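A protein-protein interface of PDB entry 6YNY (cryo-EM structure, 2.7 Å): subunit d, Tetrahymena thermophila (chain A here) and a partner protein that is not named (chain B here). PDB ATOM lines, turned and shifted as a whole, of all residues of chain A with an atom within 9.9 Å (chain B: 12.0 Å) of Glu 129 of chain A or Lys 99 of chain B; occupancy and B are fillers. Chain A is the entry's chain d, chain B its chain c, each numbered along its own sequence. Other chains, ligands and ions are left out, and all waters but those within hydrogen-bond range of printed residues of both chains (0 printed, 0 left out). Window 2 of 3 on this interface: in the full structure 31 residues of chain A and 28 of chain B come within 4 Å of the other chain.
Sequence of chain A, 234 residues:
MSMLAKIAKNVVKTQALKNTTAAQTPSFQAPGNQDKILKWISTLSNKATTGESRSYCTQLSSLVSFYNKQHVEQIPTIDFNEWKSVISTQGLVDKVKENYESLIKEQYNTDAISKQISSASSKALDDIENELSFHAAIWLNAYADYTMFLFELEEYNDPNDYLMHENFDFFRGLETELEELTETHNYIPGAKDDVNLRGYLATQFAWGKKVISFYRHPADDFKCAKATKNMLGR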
ATOM      1  N   SER A 121       0.455  29.652  21.715  1.00  0.00           N
ATOM      2  CA  SER A 121       0.264  31.083  21.515  1.00  0.00           C
ATOM      3  C   SER A 121       0.733  31.885  22.726  1.00  0.00           C
ATOM      4  O   SER A 121       1.611  32.745  22.611  1.00  0.00           O
ATOM      5  CB  SER A 121      -1.211  31.369  21.219  1.00  0.00           C
ATOM      6  OG  SER A 121      -1.636  30.697  20.045  1.00  0.00           O
ATOM      7  N   SER A 122       0.153  31.608  23.893  1.00  0.00           N
ATOM      8  CA  SER A 122       0.459  32.359  25.102  1.00  0.00           C
ATOM      9  C   SER A 122      -0.364  31.842  26.273  1.00  0.00           C
ATOM     10  O   SER A 122      -1.162  30.913  26.117  1.00  0.00           O
ATOM     11  CB  SER A 122       0.203  33.851  24.895  1.00  0.00           C
ATOM     12  OG  SER A 122       0.032  34.511  26.137  1.00  0.00           O
ATOM     13  N   LYS A 123      -0.176  32.440  27.447  1.00  0.00           N
ATOM     14  CA  LYS A 123      -1.001  32.124  28.604  1.00  0.00           C
ATOM     15  C   LYS A 123      -2.276  32.958  28.612  1.00  0.00           C
ATOM     16  O   LYS A 123      -3.380  32.411  28.678  1.00  0.00           O
ATOM     17  CB  LYS A 123      -0.200  32.352  29.890  1.00  0.00           C
ATOM     18  CG  LYS A 123      -1.031  32.625  31.137  1.00  0.00           C
ATOM     19  CD  LYS A 123      -1.995  31.490  31.444  1.00  0.00           C
ATOM     20  CE  LYS A 123      -2.737  31.736  32.747  1.00  0.00           C
ATOM     21  NZ  LYS A 123      -1.812  31.825  33.912  1.00  0.00           N
ATOM     22  N   ALA A 124      -2.139  34.284  28.542  1.00  0.00           N
ATOM     23  CA  ALA A 124      -3.311  35.147  28.619  1.00  0.00           C
ATOM     24  C   ALA A 124      -4.283  34.863  27.485  1.00  0.00           C
ATOM     25  O   ALA A 124      -5.501  34.958  27.672  1.00  0.00           O
ATOM     26  CB  ALA A 124      -2.889  36.614  28.597  1.00  0.00           C
ATOM     27  N   LEU A 125      -3.768  34.514  26.304  1.00  0.00           N
ATOM     28  CA  LEU A 125      -4.647  34.199  25.185  1.00  0.00           C
ATOM     29  C   LEU A 125      -5.464  32.948  25.470  1.00  0.00           C
ATOM     30  O   LEU A 125      -6.641  32.870  25.098  1.00  0.00           O
ATOM     31  CB  LEU A 125      -3.825  34.023  23.912  1.00  0.00           C
ATOM     32  CG  LEU A 125      -4.622  33.987  22.610  1.00  0.00           C
ATOM     33  CD1 LEU A 125      -5.229  35.346  22.311  1.00  0.00           C
ATOM     34  CD2 LEU A 125      -3.746  33.532  21.466  1.00  0.00           C
ATOM     35  N   ASP A 126      -4.860  31.958  26.127  1.00  0.00           N
ATOM     36  CA  ASP A 126      -5.603  30.757  26.484  1.00  0.00           C
ATOM     37  C   ASP A 126      -6.695  31.066  27.495  1.00  0.00           C
ATOM     38  O   ASP A 126      -7.730  30.389  27.518  1.00  0.00           O
ATOM     39  CB  ASP A 126      -4.655  29.697  27.036  1.00  0.00           C
ATOM     40  CG  ASP A 126      -3.642  29.235  26.011  1.00  0.00           C
ATOM     41  OD1 ASP A 126      -3.668  29.752  24.875  1.00  0.00           O
ATOM     42  OD2 ASP A 126      -2.820  28.354  26.340  1.00  0.00           O
ATOM     43  N   ASP A 127      -6.485  32.079  28.335  1.00  0.00           N
ATOM     44  CA  ASP A 127      -7.488  32.436  29.330  1.00  0.00           C
ATOM     45  C   ASP A 127      -8.767  32.930  28.666  1.00  0.00           C
ATOM     46  O   ASP A 127      -9.871  32.553  29.073  1.00  0.00           O
ATOM     47  CB  ASP A 127      -6.928  33.494  30.278  1.00  0.00           C
ATOM     48  CG  ASP A 127      -7.810  33.719  31.488  1.00  0.00           C
ATOM     49  OD1 ASP A 127      -8.825  33.006  31.626  1.00  0.00           O
ATOM     50  OD2 ASP A 127      -7.488  34.607  32.303  1.00  0.00           O
ATOM     51  N   ILE A 128      -8.638  33.772  27.640  1.00  0.00           N
ATOM     52  CA  ILE A 128      -9.810  34.264  26.928  1.00  0.00           C
ATOM     53  C   ILE A 128     -10.221  33.338  25.792  1.00  0.00           C
ATOM     54  O   ILE A 128     -11.392  33.354  25.385  1.00  0.00           O
ATOM     55  CB  ILE A 128      -9.574  35.685  26.389  1.00  0.00           C
ATOM     56  CG1 ILE A 128      -8.398  35.704  25.416  1.00  0.00           C
ATOM     57  CG2 ILE A 128      -9.325  36.647  27.531  1.00  0.00           C
ATOM     58  CD1 ILE A 128      -8.767  36.201  24.049  1.00  0.00           C
ATOM     59  N   GLU A 129      -9.296  32.534  25.266  1.00  0.00           N
ATOM     60  CA  GLU A 129      -9.676  31.524  24.287  1.00  0.00           C
ATOM     61  C   GLU A 129     -10.711  30.577  24.874  1.00  0.00           C
ATOM     62  O   GLU A 129     -11.623  30.125  24.172  1.00  0.00           O
ATOM     63  CB  GLU A 129      -8.438  30.757  23.826  1.00  0.00           C
ATOM     64  CG  GLU A 129      -8.715  29.506  23.006  1.00  0.00           C
ATOM     65  CD  GLU A 129      -9.416  29.804  21.701  1.00  0.00           C
ATOM     66  OE1 GLU A 129      -9.505  30.990  21.332  1.00  0.00           O
ATOM     67  OE2 GLU A 129      -9.877  28.849  21.041  1.00  0.00           O
ATOM     68  N   ASN A 130     -10.585  30.265  26.162  1.00  0.00           N
ATOM     69  CA  ASN A 130     -11.538  29.403  26.843  1.00  0.00           C
ATOM     70  C   ASN A 130     -12.696  30.179  27.449  1.00  0.00           C
ATOM     71  O   ASN A 130     -13.772  29.605  27.648  1.00  0.00           O
ATOM     72  CB  ASN A 130     -10.833  28.604  27.939  1.00  0.00           C
ATOM     73  CG  ASN A 130      -9.759  27.692  27.393  1.00  0.00           C
ATOM     74  OD1 ASN A 130      -9.847  27.222  26.260  1.00  0.00           O
ATOM     75  ND2 ASN A 130      -8.738  27.435  28.197  1.00  0.00           N
ATOM     76  N   GLU A 131     -12.503  31.463  27.748  1.00  0.00           N
ATOM     77  CA  GLU A 131     -13.591  32.274  28.276  1.00  0.00           C
ATOM     78  C   GLU A 131     -14.599  32.607  27.185  1.00  0.00           C
ATOM     79  O   GLU A 131     -15.802  32.372  27.341  1.00  0.00           O
ATOM     80  CB  GLU A 131     -13.036  33.553  28.897  1.00  0.00           C
ATOM     81  CG  GLU A 131     -14.085  34.431  29.551  1.00  0.00           C
ATOM     82  CD  GLU A 131     -13.498  35.684  30.170  1.00  0.00           C
ATOM     83  OE1 GLU A 131     -12.264  35.865  30.099  1.00  0.00           O
ATOM     84  OE2 GLU A 131     -14.272  36.490  30.727  1.00  0.00           O
ATOM     85  N   LEU A 132     -14.122  33.161  26.070  1.00  0.00           N
ATOM     86  CA  LEU A 132     -15.013  33.523  24.977  1.00  0.00           C
ATOM     87  C   LEU A 132     -15.691  32.308  24.368  1.00  0.00           C
ATOM     88  O   LEU A 132     -16.765  32.444  23.774  1.00  0.00           O
ATOM     89  CB  LEU A 132     -14.243  34.280  23.901  1.00  0.00           C
ATOM     90  CG  LEU A 132     -13.748  35.672  24.283  1.00  0.00           C
ATOM     91  CD1 LEU A 132     -12.909  36.235  23.169  1.00  0.00           C
ATOM     92  CD2 LEU A 132     -14.905  36.599  24.583  1.00  0.00           C
ATOM     93  N   SER A 133     -15.089  31.128  24.495  1.00  0.00           N
ATOM     94  CA  SER A 133     -15.727  29.919  23.994  1.00  0.00           C
ATOM     95  C   SER A 133     -16.956  29.578  24.822  1.00  0.00           C
ATOM     96  O   SER A 133     -18.041  29.345  24.278  1.00  0.00           O
ATOM     97  CB  SER A 133     -14.730  28.763  24.007  1.00  0.00           C
ATOM     98  OG  SER A 133     -13.555  29.099  23.298  1.00  0.00           O
ATOM     99  N   PHE A 134     -16.808  29.549  26.146  1.00  0.00           N
ATOM    100  CA  PHE A 134     -17.954  29.304  27.010  1.00  0.00           C
ATOM    101  C   PHE A 134     -18.971  30.427  26.886  1.00  0.00           C
ATOM    102  O   PHE A 134     -20.182  30.191  26.955  1.00  0.00           O
ATOM    103  CB  PHE A 134     -17.485  29.155  28.454  1.00  0.00           C
ATOM    104  CG  PHE A 134     -18.564  28.747  29.406  1.00  0.00           C
ATOM    105  CD1 PHE A 134     -19.044  27.453  29.415  1.00  0.00           C
ATOM    106  CD2 PHE A 134     -19.087  29.653  30.304  1.00  0.00           C
ATOM    107  CE1 PHE A 134     -20.031  27.079  30.293  1.00  0.00           C
ATOM    108  CE2 PHE A 134     -20.073  29.280  31.182  1.00  0.00           C
ATOM    109  CZ  PHE A 134     -20.544  27.993  31.177  1.00  0.00           C
ATOM    110  N   HIS A 135     -18.497  31.658  26.699  1.00  0.00           N
ATOM    111  CA  HIS A 135     -19.402  32.775  26.466  1.00  0.00           C
ATOM    112  C   HIS A 135     -20.251  32.542  25.223  1.00  0.00           C
ATOM    113  O   HIS A 135     -21.471  32.731  25.244  1.00  0.00           O
ATOM    114  CB  HIS A 135     -18.599  34.066  26.339  1.00  0.00           C
ATOM    115  CG  HIS A 135     -19.401  35.233  25.862  1.00  0.00           C
ATOM    116  ND1 HIS A 135     -19.390  35.654  24.551  1.00  0.00           N
ATOM    117  CD2 HIS A 135     -20.234  36.072  26.520  1.00  0.00           C
ATOM    118  CE1 HIS A 135     -20.184  36.700  24.421  1.00  0.00           C
ATOM    119  NE2 HIS A 135     -20.708  36.975  25.601  1.00  0.00           N
ATOM    120  N   ALA A 136     -19.618  32.126  24.125  1.00  0.00           N
ATOM    121  CA  ALA A 136     -20.366  31.880  22.897  1.00  0.00           C
ATOM    122  C   ALA A 136     -21.280  30.672  23.038  1.00  0.00           C
ATOM    123  O   ALA A 136     -22.394  30.665  22.502  1.00  0.00           O
ATOM    124  CB  ALA A 136     -19.404  31.690  21.730  1.00  0.00           C
ATOM    125  N   ALA A 137     -20.829  29.640  23.750  1.00  0.00           N
ATOM    126  CA  ALA A 137     -21.666  28.466  23.958  1.00  0.00           C
ATOM    127  C   ALA A 137     -22.923  28.810  24.737  1.00  0.00           C
ATOM    128  O   ALA A 137     -23.963  28.169  24.554  1.00  0.00           O
ATOM    129  CB  ALA A 137     -20.873  27.387  24.681  1.00  0.00           C
ATOM    130  N   ASN B  88     -27.240  22.290  19.012  1.00  0.00           N
ATOM    131  CA  ASN B  88     -26.222  22.849  19.894  1.00  0.00           C
ATOM    132  C   ASN B  88     -24.846  22.282  19.574  1.00  0.00           C
ATOM    133  O   ASN B  88     -23.883  23.030  19.378  1.00  0.00           O
ATOM    134  CB  ASN B  88     -26.587  22.578  21.350  1.00  0.00           C
ATOM    135  CG  ASN B  88     -27.732  23.433  21.832  1.00  0.00           C
ATOM    136  OD1 ASN B  88     -27.530  24.416  22.540  1.00  0.00           O
ATOM    137  ND2 ASN B  88     -28.942  23.065  21.448  1.00  0.00           N
ATOM    138  N   ASN B  89     -24.733  20.955  19.520  1.00  0.00           N
ATOM    139  CA  ASN B  89     -23.456  20.346  19.168  1.00  0.00           C
ATOM    140  C   ASN B  89     -23.033  20.714  17.755  1.00  0.00           C
ATOM    141  O   ASN B  89     -21.837  20.767  17.458  1.00  0.00           O
ATOM    142  CB  ASN B  89     -23.540  18.830  19.317  1.00  0.00           C
ATOM    143  CG  ASN B  89     -23.651  18.398  20.755  1.00  0.00           C
ATOM    144  OD1 ASN B  89     -22.652  18.292  21.465  1.00  0.00           O
ATOM    145  ND2 ASN B  89     -24.869  18.140  21.197  1.00  0.00           N
ATOM    146  N   TYR B  90     -23.998  20.964  16.871  1.00  0.00           N
ATOM    147  CA  TYR B  90     -23.669  21.404  15.523  1.00  0.00           C
ATOM    148  C   TYR B  90     -23.062  22.799  15.539  1.00  0.00           C
ATOM    149  O   TYR B  90     -22.098  23.071  14.815  1.00  0.00           O
ATOM    150  CB  TYR B  90     -24.924  21.358  14.657  1.00  0.00           C
ATOM    151  CG  TYR B  90     -24.813  22.043  13.320  1.00  0.00           C
ATOM    152  CD1 TYR B  90     -23.997  21.541  12.323  1.00  0.00           C
ATOM    153  CD2 TYR B  90     -25.551  23.180  13.046  1.00  0.00           C
ATOM    154  CE1 TYR B  90     -23.907  22.163  11.102  1.00  0.00           C
ATOM    155  CE2 TYR B  90     -25.468  23.805  11.831  1.00  0.00           C
ATOM    156  CZ  TYR B  90     -24.648  23.293  10.860  1.00  0.00           C
ATOM    157  OH  TYR B  90     -24.572  23.926   9.646  1.00  0.00           O
ATOM    158  N   TYR B  91     -23.607  23.694  16.362  1.00  0.00           N
ATOM    159  CA  TYR B  91     -23.031  25.026  16.489  1.00  0.00           C
ATOM    160  C   TYR B  91     -21.689  24.979  17.205  1.00  0.00           C
ATOM    161  O   TYR B  91     -20.760  25.711  16.844  1.00  0.00           O
ATOM    162  CB  TYR B  91     -23.995  25.946  17.234  1.00  0.00           C
ATOM    163  CG  TYR B  91     -25.240  26.342  16.476  1.00  0.00           C
ATOM    164  CD1 TYR B  91     -25.277  26.328  15.093  1.00  0.00           C
ATOM    165  CD2 TYR B  91     -26.378  26.748  17.151  1.00  0.00           C
ATOM    166  CE1 TYR B  91     -26.410  26.698  14.410  1.00  0.00           C
ATOM    167  CE2 TYR B  91     -27.511  27.118  16.477  1.00  0.00           C
ATOM    168  CZ  TYR B  91     -27.526  27.093  15.108  1.00  0.00           C
ATOM    169  OH  TYR B  91     -28.665  27.464  14.435  1.00  0.00           O
ATOM    170  N   TYR B  92     -21.568  24.132  18.226  1.00  0.00           N
ATOM    171  CA  TYR B  92     -20.332  24.076  18.998  1.00  0.00           C
ATOM    172  C   TYR B  92     -19.175  23.567  18.152  1.00  0.00           C
ATOM    173  O   TYR B  92     -18.087  24.153  18.155  1.00  0.00           O
ATOM    174  CB  TYR B  92     -20.523  23.188  20.225  1.00  0.00           C
ATOM    175  CG  TYR B  92     -21.444  23.747  21.284  1.00  0.00           C
ATOM    176  CD1 TYR B  92     -22.058  24.978  21.130  1.00  0.00           C
ATOM    177  CD2 TYR B  92     -21.690  23.041  22.449  1.00  0.00           C
ATOM    178  CE1 TYR B  92     -22.891  25.482  22.096  1.00  0.00           C
ATOM    179  CE2 TYR B  92     -22.522  23.539  23.421  1.00  0.00           C
ATOM    180  CZ  TYR B  92     -23.120  24.758  23.241  1.00  0.00           C
ATOM    181  OH  TYR B  92     -23.951  25.256  24.215  1.00  0.00           O
ATOM    182  N   ASN B  93     -19.387  22.470  17.424  1.00  0.00           N
ATOM    183  CA  ASN B  93     -18.300  21.883  16.650  1.00  0.00           C
ATOM    184  C   ASN B  93     -17.834  22.825  15.551  1.00  0.00           C
ATOM    185  O   ASN B  93     -16.629  22.971  15.318  1.00  0.00           O
ATOM    186  CB  ASN B  93     -18.743  20.553  16.052  1.00  0.00           C
ATOM    187  CG  ASN B  93     -19.177  19.558  17.104  1.00  0.00           C
ATOM    188  OD1 ASN B  93     -18.750  19.627  18.255  1.00  0.00           O
ATOM    189  ND2 ASN B  93     -20.030  18.621  16.713  1.00  0.00           N
ATOM    190  N   GLN B  94     -18.771  23.478  14.868  1.00  0.00           N
ATOM    191  CA  GLN B  94     -18.408  24.310  13.729  1.00  0.00           C
ATOM    192  C   GLN B  94     -17.680  25.574  14.163  1.00  0.00           C
ATOM    193  O   GLN B  94     -16.702  25.980  13.527  1.00  0.00           O
ATOM    194  CB  GLN B  94     -19.654  24.669  12.924  1.00  0.00           C
ATOM    195  CG  GLN B  94     -20.329  23.487  12.278  1.00  0.00           C
ATOM    196  CD  GLN B  94     -19.455  22.808  11.252  1.00  0.00           C
ATOM    197  OE1 GLN B  94     -18.601  23.437  10.630  1.00  0.00           O
ATOM    198  NE2 GLN B  94     -19.657  21.511  11.073  1.00  0.00           N
ATOM    199  N   LYS B  95     -18.133  26.207  15.242  1.00  0.00           N
ATOM    200  CA  LYS B  95     -17.610  27.507  15.640  1.00  0.00           C
ATOM    201  C   LYS B  95     -16.575  27.430  16.749  1.00  0.00           C
ATOM    202  O   LYS B  95     -15.559  28.125  16.684  1.00  0.00           O
ATOM    203  CB  LYS B  95     -18.757  28.416  16.078  1.00  0.00           C
ATOM    204  CG  LYS B  95     -19.781  28.663  14.992  1.00  0.00           C
ATOM    205  CD  LYS B  95     -20.704  29.806  15.339  1.00  0.00           C
ATOM    206  CE  LYS B  95     -20.038  31.152  15.129  1.00  0.00           C
ATOM    207  NZ  LYS B  95     -19.719  31.402  13.697  1.00  0.00           N
ATOM    208  N   LEU B  96     -16.805  26.614  17.771  1.00  0.00           N
ATOM    209  CA  LEU B  96     -15.893  26.564  18.903  1.00  0.00           C
ATOM    210  C   LEU B  96     -14.724  25.620  18.683  1.00  0.00           C
ATOM    211  O   LEU B  96     -13.682  25.785  19.327  1.00  0.00           O
ATOM    212  CB  LEU B  96     -16.641  26.144  20.170  1.00  0.00           C
ATOM    213  CG  LEU B  96     -17.876  26.966  20.531  1.00  0.00           C
ATOM    214  CD1 LEU B  96     -18.434  26.497  21.845  1.00  0.00           C
ATOM    215  CD2 LEU B  96     -17.557  28.438  20.591  1.00  0.00           C
ATOM    216  N   ILE B  97     -14.870  24.637  17.800  1.00  0.00           N
ATOM    217  CA  ILE B  97     -13.849  23.624  17.563  1.00  0.00           C
ATOM    218  C   ILE B  97     -13.236  23.771  16.175  1.00  0.00           C
ATOM    219  O   ILE B  97     -12.030  23.978  16.038  1.00  0.00           O
ATOM    220  CB  ILE B  97     -14.425  22.208  17.775  1.00  0.00           C
ATOM    221  CG1 ILE B  97     -14.892  22.055  19.222  1.00  0.00           C
ATOM    222  CG2 ILE B  97     -13.392  21.159  17.422  1.00  0.00           C
ATOM    223  CD1 ILE B  97     -15.644  20.780  19.506  1.00  0.00           C
ATOM    224  N   LEU B  98     -14.052  23.666  15.132  1.00  0.00           N
ATOM    225  CA  LEU B  98     -13.578  23.748  13.758  1.00  0.00           C
ATOM    226  C   LEU B  98     -13.529  25.173  13.226  1.00  0.00           C
ATOM    227  O   LEU B  98     -13.078  25.378  12.095  1.00  0.00           O
ATOM    228  CB  LEU B  98     -14.474  22.908  12.843  1.00  0.00           C
ATOM    229  CG  LEU B  98     -14.743  21.467  13.273  1.00  0.00           C
ATOM    230  CD1 LEU B  98     -15.678  20.809  12.283  1.00  0.00           C
ATOM    231  CD2 LEU B  98     -13.461  20.675  13.401  1.00  0.00           C
ATOM    232  N   LYS B  99     -13.970  26.155  14.004  1.00  0.00           N
ATOM    233  CA  LYS B  99     -14.043  27.534  13.537  1.00  0.00           C
ATOM    234  C   LYS B  99     -14.759  27.619  12.193  1.00  0.00           C
ATOM    235  O   LYS B  99     -15.434  28.604  11.899  1.00  0.00           O
ATOM    236  CB  LYS B  99     -12.648  28.140  13.424  1.00  0.00           C
ATOM    237  CG  LYS B  99     -12.098  28.689  14.725  1.00  0.00           C
ATOM    238  CD  LYS B  99     -11.726  27.592  15.695  1.00  0.00           C
ATOM    239  CE  LYS B  99     -11.041  28.168  16.922  1.00  0.00           C
ATOM    240  NZ  LYS B  99     -10.559  27.120  17.850  1.00  0.00           N
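The side-chain carboxylate (OE2) of Glu 129 of chain A lies within salt-bridge range of the side-chain amino group (NZ) of Lys 99 of chain B, at 3.7 Å. The side-chain hydroxyl (OH) of Tyr 92 of chain B sits at hydrogen-bond distance from the backbone carbonyl oxygen (O) of Ala 137 of chain A.
N of Ile 97 of chain B lies within hydrogen-bond range of O of Tyr 92 of chain B, at 3.3 Å. The backbone carbonyl oxygen (O) of Gln 94 of chain B is in hydrogen-bond range of the backbone NH (N) of Lys 99 of chain B (2.8 Å).
Leu 96 of chain B touches Ser 133 of chain A. CB of Ala 136 of chain A touches CD2 of Leu 96 of chain B, at 3.9 Å. Ala 137 of chain A touches Leu 96 of chain B.
Of chain B, only Lys 99 (3.7 Å) comes within 4 Å of Glu 129 of chain A. Of chain A, only Glu 129 comes within 4 Å of Lys 99 of chain B. No residue of chain B comes within 4 Å of Leu 125 of chain A. Asp 126 of chain A touches none of the printed residues of chain B. No residue of chain B comes within 4 Å of Asp 127 of chain A. Ile 128 of chain A touches none of the printed residues of chain B. No residue of chain B comes within 4 Å of Asn 130 of chain A. No residue of chain B comes within 4 Å of Leu 132 of chain A. Of chain B, only Leu 96 (3.8 Å) comes within 4 Å of Ser 133 of chain A. Printed residues of chain B within 4 Å of Ala 136 of chain A: Leu 96. Of the printed residues of chain A, Leu 96 of chain B touches Ser 133, Ala 136 and Ala 137. Of the printed residues of chain A, Tyr 92 of chain B touches Ala 137. Of the printed residues of chain B, Ala 137 of chain A touches Tyr 92 (2.9 Å) and Leu 96 (3.8 Å). The nearest residue of chain A that does not touch Lys 99 of chain B is Ser 133 of chain A (6.5 Å).
Hydrophobic or aromatic side chains of chain A that line the printed part of chain B: Ala 136 and Ala 137. Among the printed residues, 5 pairs touch across the chains.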
